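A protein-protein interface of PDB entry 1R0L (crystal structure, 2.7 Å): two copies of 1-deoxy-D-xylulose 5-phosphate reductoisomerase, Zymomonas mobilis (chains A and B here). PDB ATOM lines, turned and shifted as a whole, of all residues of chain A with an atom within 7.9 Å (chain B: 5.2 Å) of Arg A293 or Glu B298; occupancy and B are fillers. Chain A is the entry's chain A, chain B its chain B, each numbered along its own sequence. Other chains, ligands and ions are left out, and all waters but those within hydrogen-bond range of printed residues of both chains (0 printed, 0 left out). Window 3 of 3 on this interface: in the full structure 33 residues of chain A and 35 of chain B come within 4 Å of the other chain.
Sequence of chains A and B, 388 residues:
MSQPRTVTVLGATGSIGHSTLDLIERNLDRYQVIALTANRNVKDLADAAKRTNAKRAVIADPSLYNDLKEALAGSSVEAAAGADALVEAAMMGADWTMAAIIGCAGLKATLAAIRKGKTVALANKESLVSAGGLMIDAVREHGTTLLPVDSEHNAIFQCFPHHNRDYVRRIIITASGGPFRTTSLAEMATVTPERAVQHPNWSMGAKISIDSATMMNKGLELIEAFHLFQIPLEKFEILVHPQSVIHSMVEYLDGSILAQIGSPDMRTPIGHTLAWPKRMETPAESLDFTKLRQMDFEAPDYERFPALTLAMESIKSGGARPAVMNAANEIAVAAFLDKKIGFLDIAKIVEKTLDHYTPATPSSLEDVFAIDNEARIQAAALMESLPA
Leu A292 touches none of the printed residues of chain B.
Of the printed residues of chain A, Met B295 touches Arg A293 (3.7 Å), Gln A294 (3.3 Å) and Met A295 (2.9 Å).
Printed residues of chain A within 4 Å of Asp B296: Arg A293 (3.1 Å) and Gln A294 (3.0 Å).
Glu B298 touches one residue of chain A.
Of chain A, only Thr A290 comes within 4 Å of Ala B299.
Pro B300 touches none of the printed residues of chain A.
The nearest residue of chain A that does not touch Glu B298 is Thr A290 (4.1 Å).
The nearest printed residue of chain A that does not touch Asp B296 is Met A295 (5.2 Å).
CD2 of Leu B239 touches CB of Phe A289, 3.5 Å away.
O of Phe A289 touches CB of Phe B297, 3.3 Å away.
Thr A290 touches Ala B299 (OG1 to N, 3.7 Å).
O of Met B295 touches O of Arg A293, 3.7 Å away.
Asp B296 touches Arg A293 (CA to O, 3.1 Å).
NH1 of Arg A293 touches CB of Glu B298, at 3.6 Å.
Met B295 touches Gln A294.
Met A295 touches Phe B297 (CE to CE1, 3.7 Å).
Of the 10 printed residues of chain A, 5 touch a printed residue of chain B.
Hydrophobic or aromatic side chains of chain B that line the printed part of chain A: Leu B239, Met B295, Phe B297 and Ala B299.
Among the printed residues, no Asp or Glu carboxylate lies within 4 Å of a Lys or Arg side-chain nitrogen of the other chain.
The backbone NH (N) of Thr A290 is in hydrogen-bond range of the side-chain carboxylate (OD1) of Asp A288, at 2.8 Å.
The backbone carbonyl oxygen (O) of Asp B296 is in hydrogen-bond range of a ring nitrogen (ND1) of His B241.
O of Thr A290 lies within hydrogen-bond range of NE of Arg A293.
The backbone carbonyl oxygen (O) of Val B240 lies within hydrogen-bond range of the backbone NH (N) of Glu B298, at 2.9 Å.
OE1 of Glu B298 is in salt-bridge range of NH1 of Arg B181.
NE2 of Gln A294 sits close to OD1 of Asp B296 (3.2 Å).
N of Phe B297 is in hydrogen-bond range of O of Arg A293 (2.6 Å).
N of Met A295 is in hydrogen-bond range of O of Met B295.
Met A295 touches its own counterpart, Met B295.
1 position is printed for both chains.
Of the 11 pairs that touch across the chains among the printed residues, 1 has its exchanged pair printed and touching as well.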
ATOM      1  N   GLN A 243      11.395 -29.467 -37.590  1.00  0.00           N
ATOM      2  CA  GLN A 243      11.481 -30.280 -36.375  1.00  0.00           C
ATOM      3  C   GLN A 243      11.232 -31.760 -36.570  1.00  0.00           C
ATOM      4  O   GLN A 243      11.709 -32.568 -35.783  1.00  0.00           O
ATOM      5  CB  GLN A 243      10.530 -29.771 -35.290  1.00  0.00           C
ATOM      6  CG  GLN A 243      10.871 -28.395 -34.779  1.00  0.00           C
ATOM      7  CD  GLN A 243      10.666 -27.340 -35.834  1.00  0.00           C
ATOM      8  OE1 GLN A 243       9.667 -27.358 -36.554  1.00  0.00           O
ATOM      9  NE2 GLN A 243      11.598 -26.406 -35.927  1.00  0.00           N
ATOM     10  N   LEU A 287       7.218 -37.767 -26.283  1.00  0.00           N
ATOM     11  CA  LEU A 287       7.528 -36.424 -26.756  1.00  0.00           C
ATOM     12  C   LEU A 287       7.100 -35.374 -25.729  1.00  0.00           C
ATOM     13  O   LEU A 287       5.943 -35.317 -25.318  1.00  0.00           O
ATOM     14  CB  LEU A 287       6.816 -36.162 -28.083  1.00  0.00           C
ATOM     15  CG  LEU A 287       7.570 -35.313 -29.098  1.00  0.00           C
ATOM     16  CD1 LEU A 287       6.630 -34.957 -30.221  1.00  0.00           C
ATOM     17  CD2 LEU A 287       8.092 -34.064 -28.450  1.00  0.00           C
ATOM     18  N   ASP A 288       8.050 -34.550 -25.319  1.00  0.00           N
ATOM     19  CA  ASP A 288       7.800 -33.497 -24.352  1.00  0.00           C
ATOM     20  C   ASP A 288       7.576 -32.221 -25.149  1.00  0.00           C
ATOM     21  O   ASP A 288       8.535 -31.576 -25.576  1.00  0.00           O
ATOM     22  CB  ASP A 288       9.023 -33.340 -23.445  1.00  0.00           C
ATOM     23  CG  ASP A 288       8.820 -32.305 -22.363  1.00  0.00           C
ATOM     24  OD1 ASP A 288       8.236 -31.232 -22.655  1.00  0.00           O
ATOM     25  OD2 ASP A 288       9.254 -32.563 -21.219  1.00  0.00           O
ATOM     26  N   PHE A 289       6.318 -31.846 -25.348  1.00  0.00           N
ATOM     27  CA  PHE A 289       6.044 -30.652 -26.122  1.00  0.00           C
ATOM     28  C   PHE A 289       6.532 -29.373 -25.467  1.00  0.00           C
ATOM     29  O   PHE A 289       6.724 -28.362 -26.152  1.00  0.00           O
ATOM     30  CB  PHE A 289       4.567 -30.543 -26.424  1.00  0.00           C
ATOM     31  CG  PHE A 289       4.052 -31.640 -27.300  1.00  0.00           C
ATOM     32  CD1 PHE A 289       3.795 -32.904 -26.775  1.00  0.00           C
ATOM     33  CD2 PHE A 289       3.769 -31.399 -28.649  1.00  0.00           C
ATOM     34  CE1 PHE A 289       3.257 -33.910 -27.574  1.00  0.00           C
ATOM     35  CE2 PHE A 289       3.229 -32.402 -29.458  1.00  0.00           C
ATOM     36  CZ  PHE A 289       2.970 -33.656 -28.923  1.00  0.00           C
ATOM     37  N   THR A 290       6.757 -29.410 -24.157  1.00  0.00           N
ATOM     38  CA  THR A 290       7.231 -28.222 -23.450  1.00  0.00           C
ATOM     39  C   THR A 290       8.656 -27.873 -23.857  1.00  0.00           C
ATOM     40  O   THR A 290       8.995 -26.702 -24.044  1.00  0.00           O
ATOM     41  CB  THR A 290       7.197 -28.412 -21.923  1.00  0.00           C
ATOM     42  OG1 THR A 290       5.841 -28.531 -21.483  1.00  0.00           O
ATOM     43  CG2 THR A 290       7.814 -27.212 -21.235  1.00  0.00           C
ATOM     44  N   LYS A 291       9.489 -28.892 -23.998  1.00  0.00           N
ATOM     45  CA  LYS A 291      10.871 -28.677 -24.381  1.00  0.00           C
ATOM     46  C   LYS A 291      11.019 -28.426 -25.878  1.00  0.00           C
ATOM     47  O   LYS A 291      12.018 -27.855 -26.318  1.00  0.00           O
ATOM     48  CB  LYS A 291      11.696 -29.876 -23.974  1.00  0.00           C
ATOM     49  CG  LYS A 291      11.454 -30.240 -22.546  1.00  0.00           C
ATOM     50  CD  LYS A 291      12.619 -30.992 -22.017  1.00  0.00           C
ATOM     51  CE  LYS A 291      12.413 -31.380 -20.573  1.00  0.00           C
ATOM     52  NZ  LYS A 291      13.347 -32.492 -20.257  1.00  0.00           N
ATOM     53  N   LEU A 292      10.020 -28.856 -26.653  1.00  0.00           N
ATOM     54  CA  LEU A 292      10.014 -28.671 -28.101  1.00  0.00           C
ATOM     55  C   LEU A 292       9.711 -27.209 -28.361  1.00  0.00           C
ATOM     56  O   LEU A 292      10.325 -26.573 -29.219  1.00  0.00           O
ATOM     57  CB  LEU A 292       8.919 -29.521 -28.733  1.00  0.00           C
ATOM     58  CG  LEU A 292       9.070 -29.974 -30.186  1.00  0.00           C
ATOM     59  CD1 LEU A 292       7.711 -30.151 -30.772  1.00  0.00           C
ATOM     60  CD2 LEU A 292       9.815 -28.991 -31.002  1.00  0.00           C
ATOM     61  N   ARG A 293       8.721 -26.691 -27.640  1.00  0.00           N
ATOM     62  CA  ARG A 293       8.388 -25.283 -27.766  1.00  0.00           C
ATOM     63  C   ARG A 293       7.671 -24.898 -29.036  1.00  0.00           C
ATOM     64  O   ARG A 293       6.519 -24.431 -29.030  1.00  0.00           O
ATOM     65  CB  ARG A 293       9.688 -24.474 -27.707  1.00  0.00           C
ATOM     66  CG  ARG A 293       9.623 -23.306 -26.814  1.00  0.00           C
ATOM     67  CD  ARG A 293       8.941 -23.740 -25.587  1.00  0.00           C
ATOM     68  NE  ARG A 293       9.744 -23.522 -24.407  1.00  0.00           N
ATOM     69  CZ  ARG A 293       9.224 -23.074 -23.279  1.00  0.00           C
ATOM     70  NH1 ARG A 293       7.926 -22.813 -23.227  1.00  0.00           N
ATOM     71  NH2 ARG A 293       9.986 -22.888 -22.213  1.00  0.00           N
ATOM     72  N   GLN A 294       8.400 -25.088 -30.125  1.00  0.00           N
ATOM     73  CA  GLN A 294       7.919 -24.722 -31.436  1.00  0.00           C
ATOM     74  C   GLN A 294       7.900 -25.794 -32.497  1.00  0.00           C
ATOM     75  O   GLN A 294       8.583 -26.807 -32.409  1.00  0.00           O
ATOM     76  CB  GLN A 294       8.740 -23.558 -31.980  1.00  0.00           C
ATOM     77  CG  GLN A 294       8.411 -22.215 -31.386  1.00  0.00           C
ATOM     78  CD  GLN A 294       9.024 -21.092 -32.213  1.00  0.00           C
ATOM     79  OE1 GLN A 294      10.186 -21.184 -32.603  1.00  0.00           O
ATOM     80  NE2 GLN A 294       8.225 -20.063 -32.454  1.00  0.00           N
ATOM     81  N   MET A 295       7.107 -25.518 -33.521  1.00  0.00           N
ATOM     82  CA  MET A 295       6.957 -26.376 -34.680  1.00  0.00           C
ATOM     83  C   MET A 295       6.801 -25.428 -35.865  1.00  0.00           C
ATOM     84  O   MET A 295       5.983 -24.506 -35.819  1.00  0.00           O
ATOM     85  CB  MET A 295       5.707 -27.242 -34.557  1.00  0.00           C
ATOM     86  CG  MET A 295       5.890 -28.559 -33.825  1.00  0.00           C
ATOM     87  SD  MET A 295       4.371 -29.556 -33.954  1.00  0.00           S
ATOM     88  CE  MET A 295       4.516 -30.707 -32.551  1.00  0.00           C
ATOM     89  N   ARG B 181      -2.708 -15.600 -20.614  1.00  0.00           N
ATOM     90  CA  ARG B 181      -1.677 -16.609 -20.679  1.00  0.00           C
ATOM     91  C   ARG B 181      -0.316 -16.037 -20.284  1.00  0.00           C
ATOM     92  O   ARG B 181       0.494 -16.738 -19.673  1.00  0.00           O
ATOM     93  CB  ARG B 181      -1.609 -17.219 -22.087  1.00  0.00           C
ATOM     94  CG  ARG B 181      -0.441 -18.182 -22.271  1.00  0.00           C
ATOM     95  CD  ARG B 181      -0.412 -18.809 -23.657  1.00  0.00           C
ATOM     96  NE  ARG B 181      -0.182 -17.839 -24.727  1.00  0.00           N
ATOM     97  CZ  ARG B 181       1.006 -17.332 -25.052  1.00  0.00           C
ATOM     98  NH1 ARG B 181       2.101 -17.698 -24.387  1.00  0.00           N
ATOM     99  NH2 ARG B 181       1.099 -16.469 -26.055  1.00  0.00           N
ATOM    100  N   LEU B 239      -1.835 -29.157 -21.872  1.00  0.00           N
ATOM    101  CA  LEU B 239      -0.731 -28.560 -22.596  1.00  0.00           C
ATOM    102  C   LEU B 239      -1.191 -27.228 -23.194  1.00  0.00           C
ATOM    103  O   LEU B 239      -2.238 -27.170 -23.851  1.00  0.00           O
ATOM    104  CB  LEU B 239      -0.263 -29.516 -23.695  1.00  0.00           C
ATOM    105  CG  LEU B 239       0.962 -29.020 -24.479  1.00  0.00           C
ATOM    106  CD1 LEU B 239       2.162 -29.029 -23.547  1.00  0.00           C
ATOM    107  CD2 LEU B 239       1.216 -29.878 -25.735  1.00  0.00           C
ATOM    108  N   VAL B 240      -0.431 -26.158 -22.948  1.00  0.00           N
ATOM    109  CA  VAL B 240      -0.782 -24.849 -23.479  1.00  0.00           C
ATOM    110  C   VAL B 240      -0.237 -24.754 -24.893  1.00  0.00           C
ATOM    111  O   VAL B 240       0.952 -24.962 -25.133  1.00  0.00           O
ATOM    112  CB  VAL B 240      -0.215 -23.679 -22.615  1.00  0.00           C
ATOM    113  CG1 VAL B 240      -0.296 -22.384 -23.391  1.00  0.00           C
ATOM    114  CG2 VAL B 240      -1.038 -23.521 -21.321  1.00  0.00           C
ATOM    115  N   HIS B 241      -1.126 -24.424 -25.819  1.00  0.00           N
ATOM    116  CA  HIS B 241      -0.821 -24.333 -27.238  1.00  0.00           C
ATOM    117  C   HIS B 241      -1.709 -23.201 -27.773  1.00  0.00           C
ATOM    118  O   HIS B 241      -2.868 -23.414 -28.168  1.00  0.00           O
ATOM    119  CB  HIS B 241      -1.151 -25.698 -27.872  1.00  0.00           C
ATOM    120  CG  HIS B 241      -1.250 -25.679 -29.362  1.00  0.00           C
ATOM    121  ND1 HIS B 241      -0.264 -25.154 -30.168  1.00  0.00           N
ATOM    122  CD2 HIS B 241      -2.235 -26.094 -30.193  1.00  0.00           C
ATOM    123  CE1 HIS B 241      -0.641 -25.239 -31.431  1.00  0.00           C
ATOM    124  NE2 HIS B 241      -1.833 -25.805 -31.474  1.00  0.00           N
ATOM    125  N   PRO B 242      -1.173 -21.972 -27.773  1.00  0.00           N
ATOM    126  CA  PRO B 242      -1.826 -20.733 -28.220  1.00  0.00           C
ATOM    127  C   PRO B 242      -2.649 -20.836 -29.512  1.00  0.00           C
ATOM    128  O   PRO B 242      -3.855 -20.523 -29.520  1.00  0.00           O
ATOM    129  CB  PRO B 242      -0.657 -19.761 -28.354  1.00  0.00           C
ATOM    130  CG  PRO B 242       0.279 -20.220 -27.295  1.00  0.00           C
ATOM    131  CD  PRO B 242       0.246 -21.724 -27.457  1.00  0.00           C
ATOM    132  N   MET B 295       3.569 -23.219 -34.641  1.00  0.00           N
ATOM    133  CA  MET B 295       2.807 -23.832 -33.559  1.00  0.00           C
ATOM    134  C   MET B 295       3.666 -23.749 -32.294  1.00  0.00           C
ATOM    135  O   MET B 295       4.850 -24.087 -32.311  1.00  0.00           O
ATOM    136  CB  MET B 295       2.491 -25.299 -33.867  1.00  0.00           C
ATOM    137  CG  MET B 295       1.298 -25.522 -34.781  1.00  0.00           C
ATOM    138  SD  MET B 295       0.902 -27.288 -34.812  1.00  0.00           S
ATOM    139  CE  MET B 295       0.095 -27.473 -36.414  1.00  0.00           C
ATOM    140  N   ASP B 296       3.069 -23.300 -31.197  1.00  0.00           N
ATOM    141  CA  ASP B 296       3.797 -23.161 -29.938  1.00  0.00           C
ATOM    142  C   ASP B 296       3.245 -23.993 -28.795  1.00  0.00           C
ATOM    143  O   ASP B 296       2.034 -24.206 -28.700  1.00  0.00           O
ATOM    144  CB  ASP B 296       3.814 -21.691 -29.540  1.00  0.00           C
ATOM    145  CG  ASP B 296       4.531 -20.841 -30.555  1.00  0.00           C
ATOM    146  OD1 ASP B 296       5.760 -21.039 -30.697  1.00  0.00           O
ATOM    147  OD2 ASP B 296       3.877 -19.990 -31.214  1.00  0.00           O
ATOM    148  N   PHE B 297       4.138 -24.458 -27.926  1.00  0.00           N
ATOM    149  CA  PHE B 297       3.726 -25.263 -26.771  1.00  0.00           C
ATOM    150  C   PHE B 297       4.463 -24.905 -25.488  1.00  0.00           C
ATOM    151  O   PHE B 297       5.670 -24.666 -25.502  1.00  0.00           O
ATOM    152  CB  PHE B 297       3.934 -26.760 -27.029  1.00  0.00           C
ATOM    153  CG  PHE B 297       3.408 -27.221 -28.338  1.00  0.00           C
ATOM    154  CD1 PHE B 297       4.196 -27.140 -29.488  1.00  0.00           C
ATOM    155  CD2 PHE B 297       2.120 -27.731 -28.434  1.00  0.00           C
ATOM    156  CE1 PHE B 297       3.709 -27.563 -30.721  1.00  0.00           C
ATOM    157  CE2 PHE B 297       1.616 -28.161 -29.665  1.00  0.00           C
ATOM    158  CZ  PHE B 297       2.413 -28.077 -30.809  1.00  0.00           C
ATOM    159  N   GLU B 298       3.732 -24.893 -24.377  1.00  0.00           N
ATOM    160  CA  GLU B 298       4.310 -24.585 -23.071  1.00  0.00           C
ATOM    161  C   GLU B 298       3.483 -25.274 -21.980  1.00  0.00           C
ATOM    162  O   GLU B 298       2.350 -25.693 -22.213  1.00  0.00           O
ATOM    163  CB  GLU B 298       4.335 -23.065 -22.851  1.00  0.00           C
ATOM    164  CG  GLU B 298       2.968 -22.431 -22.839  1.00  0.00           C
ATOM    165  CD  GLU B 298       3.007 -20.919 -22.914  1.00  0.00           C
ATOM    166  OE1 GLU B 298       3.406 -20.388 -23.975  1.00  0.00           O
ATOM    167  OE2 GLU B 298       2.633 -20.262 -21.918  1.00  0.00           O
ATOM    168  N   ALA B 299       4.045 -25.401 -20.786  1.00  0.00           N
ATOM    169  CA  ALA B 299       3.319 -26.051 -19.702  1.00  0.00           C
ATOM    170  C   ALA B 299       2.368 -25.065 -19.070  1.00  0.00           C
ATOM    171  O   ALA B 299       2.622 -23.866 -19.065  1.00  0.00           O
ATOM    172  CB  ALA B 299       4.293 -26.585 -18.635  1.00  0.00           C
ATOM    173  N   PRO B 300       1.239 -25.562 -18.542  1.00  0.00           N
ATOM    174  CA  PRO B 300       0.258 -24.681 -17.897  1.00  0.00           C
ATOM    175  C   PRO B 300       0.847 -24.208 -16.561  1.00  0.00           C
ATOM    176  O   PRO B 300       1.605 -24.941 -15.918  1.00  0.00           O
ATOM    177  CB  PRO B 300      -0.951 -25.591 -17.718  1.00  0.00           C
ATOM    178  CG  PRO B 300      -0.294 -26.952 -17.483  1.00  0.00           C
ATOM    179  CD  PRO B 300       0.792 -26.972 -18.525  1.00  0.00           C
